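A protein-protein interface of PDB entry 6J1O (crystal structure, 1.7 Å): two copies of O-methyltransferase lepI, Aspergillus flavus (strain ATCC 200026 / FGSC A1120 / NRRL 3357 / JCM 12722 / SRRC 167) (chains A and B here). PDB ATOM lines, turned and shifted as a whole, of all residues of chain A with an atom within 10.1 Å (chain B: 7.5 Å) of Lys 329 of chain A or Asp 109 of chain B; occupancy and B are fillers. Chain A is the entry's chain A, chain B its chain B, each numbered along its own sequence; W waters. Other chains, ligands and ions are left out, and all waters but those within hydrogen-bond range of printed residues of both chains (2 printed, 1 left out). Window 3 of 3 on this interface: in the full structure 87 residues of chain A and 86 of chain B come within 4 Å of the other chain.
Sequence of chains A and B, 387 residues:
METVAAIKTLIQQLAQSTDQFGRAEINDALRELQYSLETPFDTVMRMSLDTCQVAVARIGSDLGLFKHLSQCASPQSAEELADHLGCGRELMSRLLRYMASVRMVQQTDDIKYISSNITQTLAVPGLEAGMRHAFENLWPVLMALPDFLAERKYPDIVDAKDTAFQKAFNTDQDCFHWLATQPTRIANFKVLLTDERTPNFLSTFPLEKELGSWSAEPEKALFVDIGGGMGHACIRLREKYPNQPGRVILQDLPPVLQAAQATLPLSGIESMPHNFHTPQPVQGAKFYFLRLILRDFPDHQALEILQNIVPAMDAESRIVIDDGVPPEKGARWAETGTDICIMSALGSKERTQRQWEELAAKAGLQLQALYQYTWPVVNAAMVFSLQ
Among the printed residues, merely in contact across the chains: Lys 329 of chain A with Gln 107 of chain B (3.5 Å), Lys 329 of chain A with Ile 111 of chain B (3.9 Å), Thr 336 of chain A with Arg 97 of chain B (3.98 Å) and Glu 328 of chain A with Ile 111 of chain B (3.99 Å).
No position is printed for both chains. Of the 7 pairs that touch across the chains among the printed residues, none has its exchanged pair printed and touching as well.
The backbone NH of Gly 330 of chain A is in hydrogen-bond range of the side-chain amide oxygen of Gln 107 of chain B (2.8 Å). O of Asp 109 of chain B sits at hydrogen-bond distance from NZ of Lys 329 of chain A (2.7 Å). The backbone carbonyl oxygen (O) of Glu 328 of chain A is in hydrogen-bond range of the guanidinium group (NH1) of Arg 97 of chain B, at 2.7 Å.
The backbone carbonyl oxygen (O) of Arg 332 of chain A sits at hydrogen-bond distance from the side-chain hydroxyl (OG1) of Thr 336 of chain A (3.3 Å). The backbone carbonyl oxygen (O) of Trp 333 of chain A sits at hydrogen-bond distance from the side-chain hydroxyl (OG1) of Thr 336 of chain A. NE2 of Gln 107 of chain B is in hydrogen-bond range of OH of Tyr 113 of chain B, 3.0 Å away.
Water W1 lies within hydrogen-bond range of O of Arg 97 of chain B and O of Ala 331 of chain A. Water W2 bridges the guanidinium group of Arg 97 of chain B (2.9 Å) and the side-chain carboxylate of Glu 328 of chain A (2.9 Å).
Hydrophobic or aromatic side chains of chain B that line the printed part of chain A: Ile 111. Among the printed residues, 7 pairs touch across the chains. Among the printed residues, no Asp or Glu carboxylate lies within 4 Å of a Lys or Arg side-chain nitrogen of the other chain.
Of the printed residues of chain B, Glu 328 of chain A touches Arg 97 (2.7 Å) and Ile 111 (3.99 Å). Of the printed residues of chain B, Lys 329 of chain A touches Gln 107 (3.5 Å), Asp 109 (2.7 Å) and Ile 111 (3.9 Å). Of the printed residues of chain A, Arg 97 of chain B touches Glu 328 and Thr 336. Printed residues of chain A within 4 Å of Gln 107 of chain B: Lys 329 and Gly 330. No residue of chain A comes within 4 Å of Thr 108 of chain B. Asp 109 of chain B touches just one residue of chain A: Lys 329 (2.7 Å). No residue of chain A comes within 4 Å of Asp 110 of chain B. Printed residues of chain A within 4 Å of Ile 111 of chain B: Glu 328 (3.99 Å) and Lys 329 (3.9 Å). The nearest residue of chain B that does not touch Lys 329 of chain A is Arg 97 of chain B (4.6 Å).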
ATOM      1  N   VAL A 325      19.983 -24.980  -4.426  1.00  0.00           N
ATOM      2  CA  VAL A 325      20.300 -23.557  -4.554  1.00  0.00           C
ATOM      3  C   VAL A 325      18.992 -22.789  -4.708  1.00  0.00           C
ATOM      4  O   VAL A 325      18.693 -22.266  -5.794  1.00  0.00           O
ATOM      5  CB  VAL A 325      21.256 -23.293  -5.730  1.00  0.00           C
ATOM      6  CG1 VAL A 325      21.809 -21.874  -5.647  1.00  0.00           C
ATOM      7  CG2 VAL A 325      22.397 -24.305  -5.743  1.00  0.00           C
ATOM      8  N   PRO A 326      18.185 -22.694  -3.655  1.00  0.00           N
ATOM      9  CA  PRO A 326      16.888 -22.044  -3.793  1.00  0.00           C
ATOM     10  C   PRO A 326      17.058 -20.582  -4.152  1.00  0.00           C
ATOM     11  O   PRO A 326      18.090 -19.962  -3.834  1.00  0.00           O
ATOM     12  CB  PRO A 326      16.259 -22.213  -2.401  1.00  0.00           C
ATOM     13  CG  PRO A 326      17.418 -22.417  -1.483  1.00  0.00           C
ATOM     14  CD  PRO A 326      18.400 -23.214  -2.295  1.00  0.00           C
ATOM     15  N   PRO A 327      16.065 -19.987  -4.810  1.00  0.00           N
ATOM     16  CA  PRO A 327      16.173 -18.583  -5.222  1.00  0.00           C
ATOM     17  C   PRO A 327      16.010 -17.633  -4.044  1.00  0.00           C
ATOM     18  O   PRO A 327      15.566 -18.002  -2.956  1.00  0.00           O
ATOM     19  CB  PRO A 327      15.025 -18.424  -6.222  1.00  0.00           C
ATOM     20  CG  PRO A 327      13.987 -19.402  -5.743  1.00  0.00           C
ATOM     21  CD  PRO A 327      14.807 -20.603  -5.277  1.00  0.00           C
ATOM     22  N   GLU A 328      16.378 -16.372  -4.300  1.00  0.00           N
ATOM     23  CA  GLU A 328      16.213 -15.313  -3.305  1.00  0.00           C
ATOM     24  C   GLU A 328      14.755 -15.109  -2.921  1.00  0.00           C
ATOM     25  O   GLU A 328      14.460 -14.755  -1.773  1.00  0.00           O
ATOM     26  CB  GLU A 328      16.789 -14.001  -3.837  1.00  0.00           C
ATOM     27  CG  GLU A 328      18.283 -14.019  -4.115  1.00  0.00           C
ATOM     28  CD  GLU A 328      19.101 -13.755  -2.869  1.00  0.00           C
ATOM     29  OE1 GLU A 328      18.642 -12.968  -2.013  1.00  0.00           O
ATOM     30  OE2 GLU A 328      20.206 -14.325  -2.745  1.00  0.00           O
ATOM     31  N   LYS A 329      13.838 -15.309  -3.863  1.00  0.00           N
ATOM     32  CA  LYS A 329      12.418 -15.150  -3.602  1.00  0.00           C
ATOM     33  C   LYS A 329      11.646 -16.148  -4.451  1.00  0.00           C
ATOM     34  O   LYS A 329      12.158 -16.687  -5.437  1.00  0.00           O
ATOM     35  CB  LYS A 329      11.955 -13.717  -3.893  1.00  0.00           C
ATOM     36  CG  LYS A 329      12.119 -13.320  -5.345  1.00  0.00           C
ATOM     37  CD  LYS A 329      11.818 -11.842  -5.568  1.00  0.00           C
ATOM     38  CE  LYS A 329      11.705 -11.531  -7.055  1.00  0.00           C
ATOM     39  NZ  LYS A 329      11.528 -10.076  -7.321  1.00  0.00           N
ATOM     40  N   GLY A 330      10.405 -16.400  -4.045  1.00  0.00           N
ATOM     41  CA  GLY A 330       9.561 -17.337  -4.759  1.00  0.00           C
ATOM     42  C   GLY A 330       9.983 -18.788  -4.649  1.00  0.00           C
ATOM     43  O   GLY A 330       9.670 -19.579  -5.540  1.00  0.00           O
ATOM     44  N   ALA A 331      10.684 -19.159  -3.579  1.00  0.00           N
ATOM     45  CA  ALA A 331      11.129 -20.539  -3.424  1.00  0.00           C
ATOM     46  C   ALA A 331       9.937 -21.477  -3.245  1.00  0.00           C
ATOM     47  O   ALA A 331       8.910 -21.105  -2.671  1.00  0.00           O
ATOM     48  CB  ALA A 331      12.086 -20.661  -2.238  1.00  0.00           C
ATOM     49  N   ARG A 332      10.083 -22.704  -3.744  1.00  0.00           N
ATOM     50  CA  ARG A 332       9.013 -23.698  -3.754  1.00  0.00           C
ATOM     51  C   ARG A 332       8.973 -24.489  -2.445  1.00  0.00           C
ATOM     52  O   ARG A 332       9.934 -24.519  -1.678  1.00  0.00           O
ATOM     53  CB  ARG A 332       9.181 -24.670  -4.926  1.00  0.00           C
ATOM     54  CG  ARG A 332       9.443 -24.022  -6.283  1.00  0.00           C
ATOM     55  CD  ARG A 332       8.233 -23.257  -6.767  1.00  0.00           C
ATOM     56  NE  ARG A 332       8.420 -22.649  -8.092  1.00  0.00           N
ATOM     57  CZ  ARG A 332       7.708 -22.954  -9.180  1.00  0.00           C
ATOM     58  NH1 ARG A 332       6.763 -23.888  -9.138  1.00  0.00           N
ATOM     59  NH2 ARG A 332       7.944 -22.322 -10.324  1.00  0.00           N
ATOM     60  N   TRP A 333       7.833 -25.153  -2.209  1.00  0.00           N
ATOM     61  CA  TRP A 333       7.627 -25.838  -0.930  1.00  0.00           C
ATOM     62  C   TRP A 333       8.655 -26.939  -0.698  1.00  0.00           C
ATOM     63  O   TRP A 333       9.030 -27.203   0.452  1.00  0.00           O
ATOM     64  CB  TRP A 333       6.203 -26.407  -0.847  1.00  0.00           C
ATOM     65  CG  TRP A 333       5.910 -27.465  -1.874  1.00  0.00           C
ATOM     66  CD1 TRP A 333       5.356 -27.279  -3.113  1.00  0.00           C
ATOM     67  CD2 TRP A 333       6.174 -28.871  -1.762  1.00  0.00           C
ATOM     68  NE1 TRP A 333       5.262 -28.482  -3.775  1.00  0.00           N
ATOM     69  CE2 TRP A 333       5.757 -29.474  -2.967  1.00  0.00           C
ATOM     70  CE3 TRP A 333       6.727 -29.678  -0.761  1.00  0.00           C
ATOM     71  CZ2 TRP A 333       5.874 -30.850  -3.197  1.00  0.00           C
ATOM     72  CZ3 TRP A 333       6.850 -31.048  -0.998  1.00  0.00           C
ATOM     73  CH2 TRP A 333       6.421 -31.614  -2.201  1.00  0.00           C
ATOM     74  N   GLU A 335      11.762 -26.941  -1.377  1.00  0.00           N
ATOM     75  CA  GLU A 335      13.062 -26.420  -0.996  1.00  0.00           C
ATOM     76  C   GLU A 335      12.979 -25.450   0.185  1.00  0.00           C
ATOM     77  O   GLU A 335      14.012 -24.923   0.606  1.00  0.00           O
ATOM     78  CB  GLU A 335      13.756 -25.765  -2.213  1.00  0.00           C
ATOM     79  CG  GLU A 335      13.083 -24.512  -2.730  1.00  0.00           C
ATOM     80  CD  GLU A 335      13.482 -24.116  -4.146  1.00  0.00           C
ATOM     81  OE1 GLU A 335      12.702 -23.361  -4.759  1.00  0.00           O
ATOM     82  OE2 GLU A 335      14.548 -24.549  -4.654  1.00  0.00           O
ATOM     83  N   THR A 336      11.793 -25.222   0.745  1.00  0.00           N
ATOM     84  CA  THR A 336      11.651 -24.510   2.018  1.00  0.00           C
ATOM     85  C   THR A 336      11.244 -25.428   3.161  1.00  0.00           C
ATOM     86  O   THR A 336      11.684 -25.229   4.307  1.00  0.00           O
ATOM     87  CB  THR A 336      10.615 -23.378   1.908  1.00  0.00           C
ATOM     88  OG1 THR A 336       9.363 -23.928   1.489  1.00  0.00           O
ATOM     89  CG2 THR A 336      11.063 -22.300   0.909  1.00  0.00           C
ATOM     90  N   THR A 352      21.007 -20.042  -0.535  1.00  0.00           N
ATOM     91  CA  THR A 352      20.960 -19.403  -1.840  1.00  0.00           C
ATOM     92  C   THR A 352      22.343 -19.424  -2.479  1.00  0.00           C
ATOM     93  O   THR A 352      23.348 -19.732  -1.832  1.00  0.00           O
ATOM     94  CB  THR A 352      20.502 -17.947  -1.733  1.00  0.00           C
ATOM     95  OG1 THR A 352      21.458 -17.202  -0.959  1.00  0.00           O
ATOM     96  CG2 THR A 352      19.137 -17.863  -1.079  1.00  0.00           C
ATOM     97  N   GLN A 353      22.387 -19.067  -3.763  1.00  0.00           N
ATOM     98  CA  GLN A 353      23.677 -18.966  -4.443  1.00  0.00           C
ATOM     99  C   GLN A 353      24.605 -17.995  -3.721  1.00  0.00           C
ATOM    100  O   GLN A 353      25.784 -18.297  -3.506  1.00  0.00           O
ATOM    101  CB  GLN A 353      23.491 -18.543  -5.897  1.00  0.00           C
ATOM    102  CG  GLN A 353      24.808 -18.533  -6.664  1.00  0.00           C
ATOM    103  CD  GLN A 353      24.675 -17.922  -8.041  1.00  0.00           C
ATOM    104  OE1 GLN A 353      23.685 -18.142  -8.736  1.00  0.00           O
ATOM    105  NE2 GLN A 353      25.673 -17.138  -8.439  1.00  0.00           N
ATOM    106  N   ARG A 354      24.091 -16.828  -3.318  1.00  0.00           N
ATOM    107  CA  ARG A 354      24.945 -15.871  -2.619  1.00  0.00           C
ATOM    108  C   ARG A 354      25.452 -16.435  -1.296  1.00  0.00           C
ATOM    109  O   ARG A 354      26.601 -16.189  -0.905  1.00  0.00           O
ATOM    110  CB  ARG A 354      24.197 -14.557  -2.389  1.00  0.00           C
ATOM    111  CG  ARG A 354      23.879 -13.818  -3.673  1.00  0.00           C
ATOM    112  CD  ARG A 354      23.036 -12.576  -3.410  1.00  0.00           C
ATOM    113  NE  ARG A 354      23.810 -11.529  -2.743  1.00  0.00           N
ATOM    114  CZ  ARG A 354      24.617 -10.687  -3.377  1.00  0.00           C
ATOM    115  NH1 ARG A 354      24.762 -10.777  -4.693  1.00  0.00           N
ATOM    116  NH2 ARG A 354      25.286  -9.762  -2.698  1.00  0.00           N
ATOM    117  N   GLN A 355      24.623 -17.211  -0.601  1.00  0.00           N
ATOM    118  CA  GLN A 355      25.067 -17.796   0.661  1.00  0.00           C
ATOM    119  C   GLN A 355      26.118 -18.883   0.429  1.00  0.00           C
ATOM    120  O   GLN A 355      27.078 -19.005   1.206  1.00  0.00           O
ATOM    121  CB  GLN A 355      23.862 -18.326   1.428  1.00  0.00           C
ATOM    122  CG  GLN A 355      23.002 -17.182   1.981  1.00  0.00           C
ATOM    123  CD  GLN A 355      21.659 -17.633   2.501  1.00  0.00           C
ATOM    124  OE1 GLN A 355      21.118 -18.648   2.071  1.00  0.00           O
ATOM    125  NE2 GLN A 355      21.097 -16.859   3.426  1.00  0.00           N
ATOM    126  N   PRO A 376      11.339 -26.999 -11.200  1.00  0.00           N
ATOM    127  CA  PRO A 376      11.613 -25.638 -10.732  1.00  0.00           C
ATOM    128  C   PRO A 376      12.401 -25.585  -9.421  1.00  0.00           C
ATOM    129  O   PRO A 376      13.014 -24.556  -9.140  1.00  0.00           O
ATOM    130  CB  PRO A 376      10.205 -25.055 -10.540  1.00  0.00           C
ATOM    131  CG  PRO A 376       9.371 -26.234 -10.219  1.00  0.00           C
ATOM    132  CD  PRO A 376       9.917 -27.358 -11.042  1.00  0.00           C
ATOM    133  N   VAL A 378      15.559 -25.980  -7.428  1.00  0.00           N
ATOM    134  CA  VAL A 378      16.905 -25.820  -7.978  1.00  0.00           C
ATOM    135  C   VAL A 378      17.861 -26.792  -7.292  1.00  0.00           C
ATOM    136  O   VAL A 378      18.179 -26.630  -6.114  1.00  0.00           O
ATOM    137  CB  VAL A 378      17.414 -24.383  -7.815  1.00  0.00           C
ATOM    138  CG1 VAL A 378      18.773 -24.237  -8.511  1.00  0.00           C
ATOM    139  CG2 VAL A 378      16.410 -23.383  -8.339  1.00  0.00           C
ATOM    140  N   ARG B  97       9.353 -17.514   4.501  1.00  0.00           N
ATOM    141  CA  ARG B  97       9.609 -18.082   3.178  1.00  0.00           C
ATOM    142  C   ARG B  97       8.875 -19.407   3.000  1.00  0.00           C
ATOM    143  O   ARG B  97       8.268 -19.661   1.942  1.00  0.00           O
ATOM    144  CB  ARG B  97      11.113 -18.241   2.958  1.00  0.00           C
ATOM    145  CG  ARG B  97      11.805 -16.889   2.835  1.00  0.00           C
ATOM    146  CD  ARG B  97      13.315 -16.987   2.926  1.00  0.00           C
ATOM    147  NE  ARG B  97      13.924 -15.659   3.030  1.00  0.00           N
ATOM    148  CZ  ARG B  97      14.174 -14.865   1.992  1.00  0.00           C
ATOM    149  NH1 ARG B  97      13.864 -15.256   0.765  1.00  0.00           N
ATOM    150  NH2 ARG B  97      14.727 -13.675   2.177  1.00  0.00           N
ATOM    151  N   GLN B 107       4.073 -13.670  -0.479  1.00  0.00           N
ATOM    152  CA  GLN B 107       5.324 -12.937  -0.604  1.00  0.00           C
ATOM    153  C   GLN B 107       5.235 -12.011  -1.809  1.00  0.00           C
ATOM    154  O   GLN B 107       4.847 -12.445  -2.898  1.00  0.00           O
ATOM    155  CB  GLN B 107       6.493 -13.911  -0.763  1.00  0.00           C
ATOM    156  CG  GLN B 107       7.869 -13.284  -0.691  1.00  0.00           C
ATOM    157  CD  GLN B 107       8.951 -14.276  -1.083  1.00  0.00           C
ATOM    158  OE1 GLN B 107       9.029 -14.691  -2.239  1.00  0.00           O
ATOM    159  NE2 GLN B 107       9.778 -14.670  -0.119  1.00  0.00           N
ATOM    160  N   THR B 108       5.584 -10.743  -1.615  1.00  0.00           N
ATOM    161  CA  THR B 108       5.542  -9.776  -2.702  1.00  0.00           C
ATOM    162  C   THR B 108       6.840  -9.820  -3.507  1.00  0.00           C
ATOM    163  O   THR B 108       7.831 -10.434  -3.111  1.00  0.00           O
ATOM    164  CB  THR B 108       5.306  -8.362  -2.169  1.00  0.00           C
ATOM    165  OG1 THR B 108       6.435  -7.951  -1.390  1.00  0.00           O
ATOM    166  CG2 THR B 108       4.046  -8.310  -1.310  1.00  0.00           C
ATOM    167  N   ASP B 109       6.830  -9.128  -4.650  1.00  0.00           N
ATOM    168  CA  ASP B 109       8.010  -9.103  -5.512  1.00  0.00           C
ATOM    169  C   ASP B 109       9.213  -8.444  -4.850  1.00  0.00           C
ATOM    170  O   ASP B 109      10.347  -8.681  -5.284  1.00  0.00           O
ATOM    171  CB  ASP B 109       7.684  -8.396  -6.828  1.00  0.00           C
ATOM    172  CG  ASP B 109       6.940  -9.292  -7.800  1.00  0.00           C
ATOM    173  OD1 ASP B 109       6.437 -10.351  -7.370  1.00  0.00           O
ATOM    174  OD2 ASP B 109       6.870  -8.943  -8.998  1.00  0.00           O
ATOM    175  N   ASP B 110       9.005  -7.620  -3.822  1.00  0.00           N
ATOM    176  CA  ASP B 110      10.104  -7.022  -3.073  1.00  0.00           C
ATOM    177  C   ASP B 110      10.381  -7.754  -1.762  1.00  0.00           C
ATOM    178  O   ASP B 110      10.967  -7.170  -0.844  1.00  0.00           O
ATOM    179  CB  ASP B 110       9.832  -5.540  -2.810  1.00  0.00           C
ATOM    180  CG  ASP B 110       8.478  -5.295  -2.183  1.00  0.00           C
ATOM    181  OD1 ASP B 110       7.556  -6.102  -2.422  1.00  0.00           O
ATOM    182  OD2 ASP B 110       8.335  -4.286  -1.461  1.00  0.00           O
ATOM    183  N   ILE B 111       9.967  -9.019  -1.664  1.00  0.00           N
ATOM    184  CA  ILE B 111      10.241  -9.886  -0.518  1.00  0.00           C
ATOM    185  C   ILE B 111       9.690  -9.270   0.762  1.00  0.00           C
ATOM    186  O   ILE B 111      10.356  -9.247   1.804  1.00  0.00           O
ATOM    187  CB  ILE B 111      11.744 -10.203  -0.397  1.00  0.00           C
ATOM    188  CG1 ILE B 111      12.357 -10.405  -1.783  1.00  0.00           C
ATOM    189  CG2 ILE B 111      11.961 -11.466   0.435  1.00  0.00           C
ATOM    190  CD1 ILE B 111      13.815 -10.815  -1.748  1.00  0.00           C
ATOM    191  N   LYS B 112       8.469  -8.764   0.690  1.00  0.00           N
ATOM    192  CA  LYS B 112       7.687  -8.435   1.866  1.00  0.00           C
ATOM    193  C   LYS B 112       6.477  -9.362   1.904  1.00  0.00           C
ATOM    194  O   LYS B 112       6.297 -10.211   1.026  1.00  0.00           O
ATOM    195  CB  LYS B 112       7.293  -6.957   1.857  1.00  0.00           C
ATOM    196  CG  LYS B 112       8.501  -6.024   1.786  1.00  0.00           C
ATOM    197  CD  LYS B 112       8.086  -4.563   1.852  1.00  0.00           C
ATOM    198  CE  LYS B 112       9.272  -3.636   1.611  1.00  0.00           C
ATOM    199  NZ  LYS B 112      10.322  -3.790   2.651  1.00  0.00           N
ATOM    200  N   TYR B 113       5.648  -9.215   2.934  1.00  0.00           N
ATOM    201  CA  TYR B 113       4.626 -10.219   3.204  1.00  0.00           C
ATOM    202  C   TYR B 113       3.269  -9.587   3.467  1.00  0.00           C
ATOM    203  O   TYR B 113       3.163  -8.580   4.172  1.00  0.00           O
ATOM    204  CB  TYR B 113       5.065 -11.110   4.379  1.00  0.00           C
ATOM    205  CG  TYR B 113       6.304 -11.887   3.998  1.00  0.00           C
ATOM    206  CD1 TYR B 113       6.209 -13.068   3.269  1.00  0.00           C
ATOM    207  CD2 TYR B 113       7.570 -11.405   4.301  1.00  0.00           C
ATOM    208  CE1 TYR B 113       7.344 -13.763   2.882  1.00  0.00           C
ATOM    209  CE2 TYR B 113       8.703 -12.090   3.921  1.00  0.00           C
ATOM    210  CZ  TYR B 113       8.584 -13.271   3.217  1.00  0.00           C
ATOM    211  OH  TYR B 113       9.718 -13.954   2.833  1.00  0.00           O
HETATM  212  O   HOH W   1       8.908 -18.660  -0.558  1.00  0.00           O
HETATM  213  O   HOH W   2      16.412 -13.159  -0.112  1.00  0.00           O
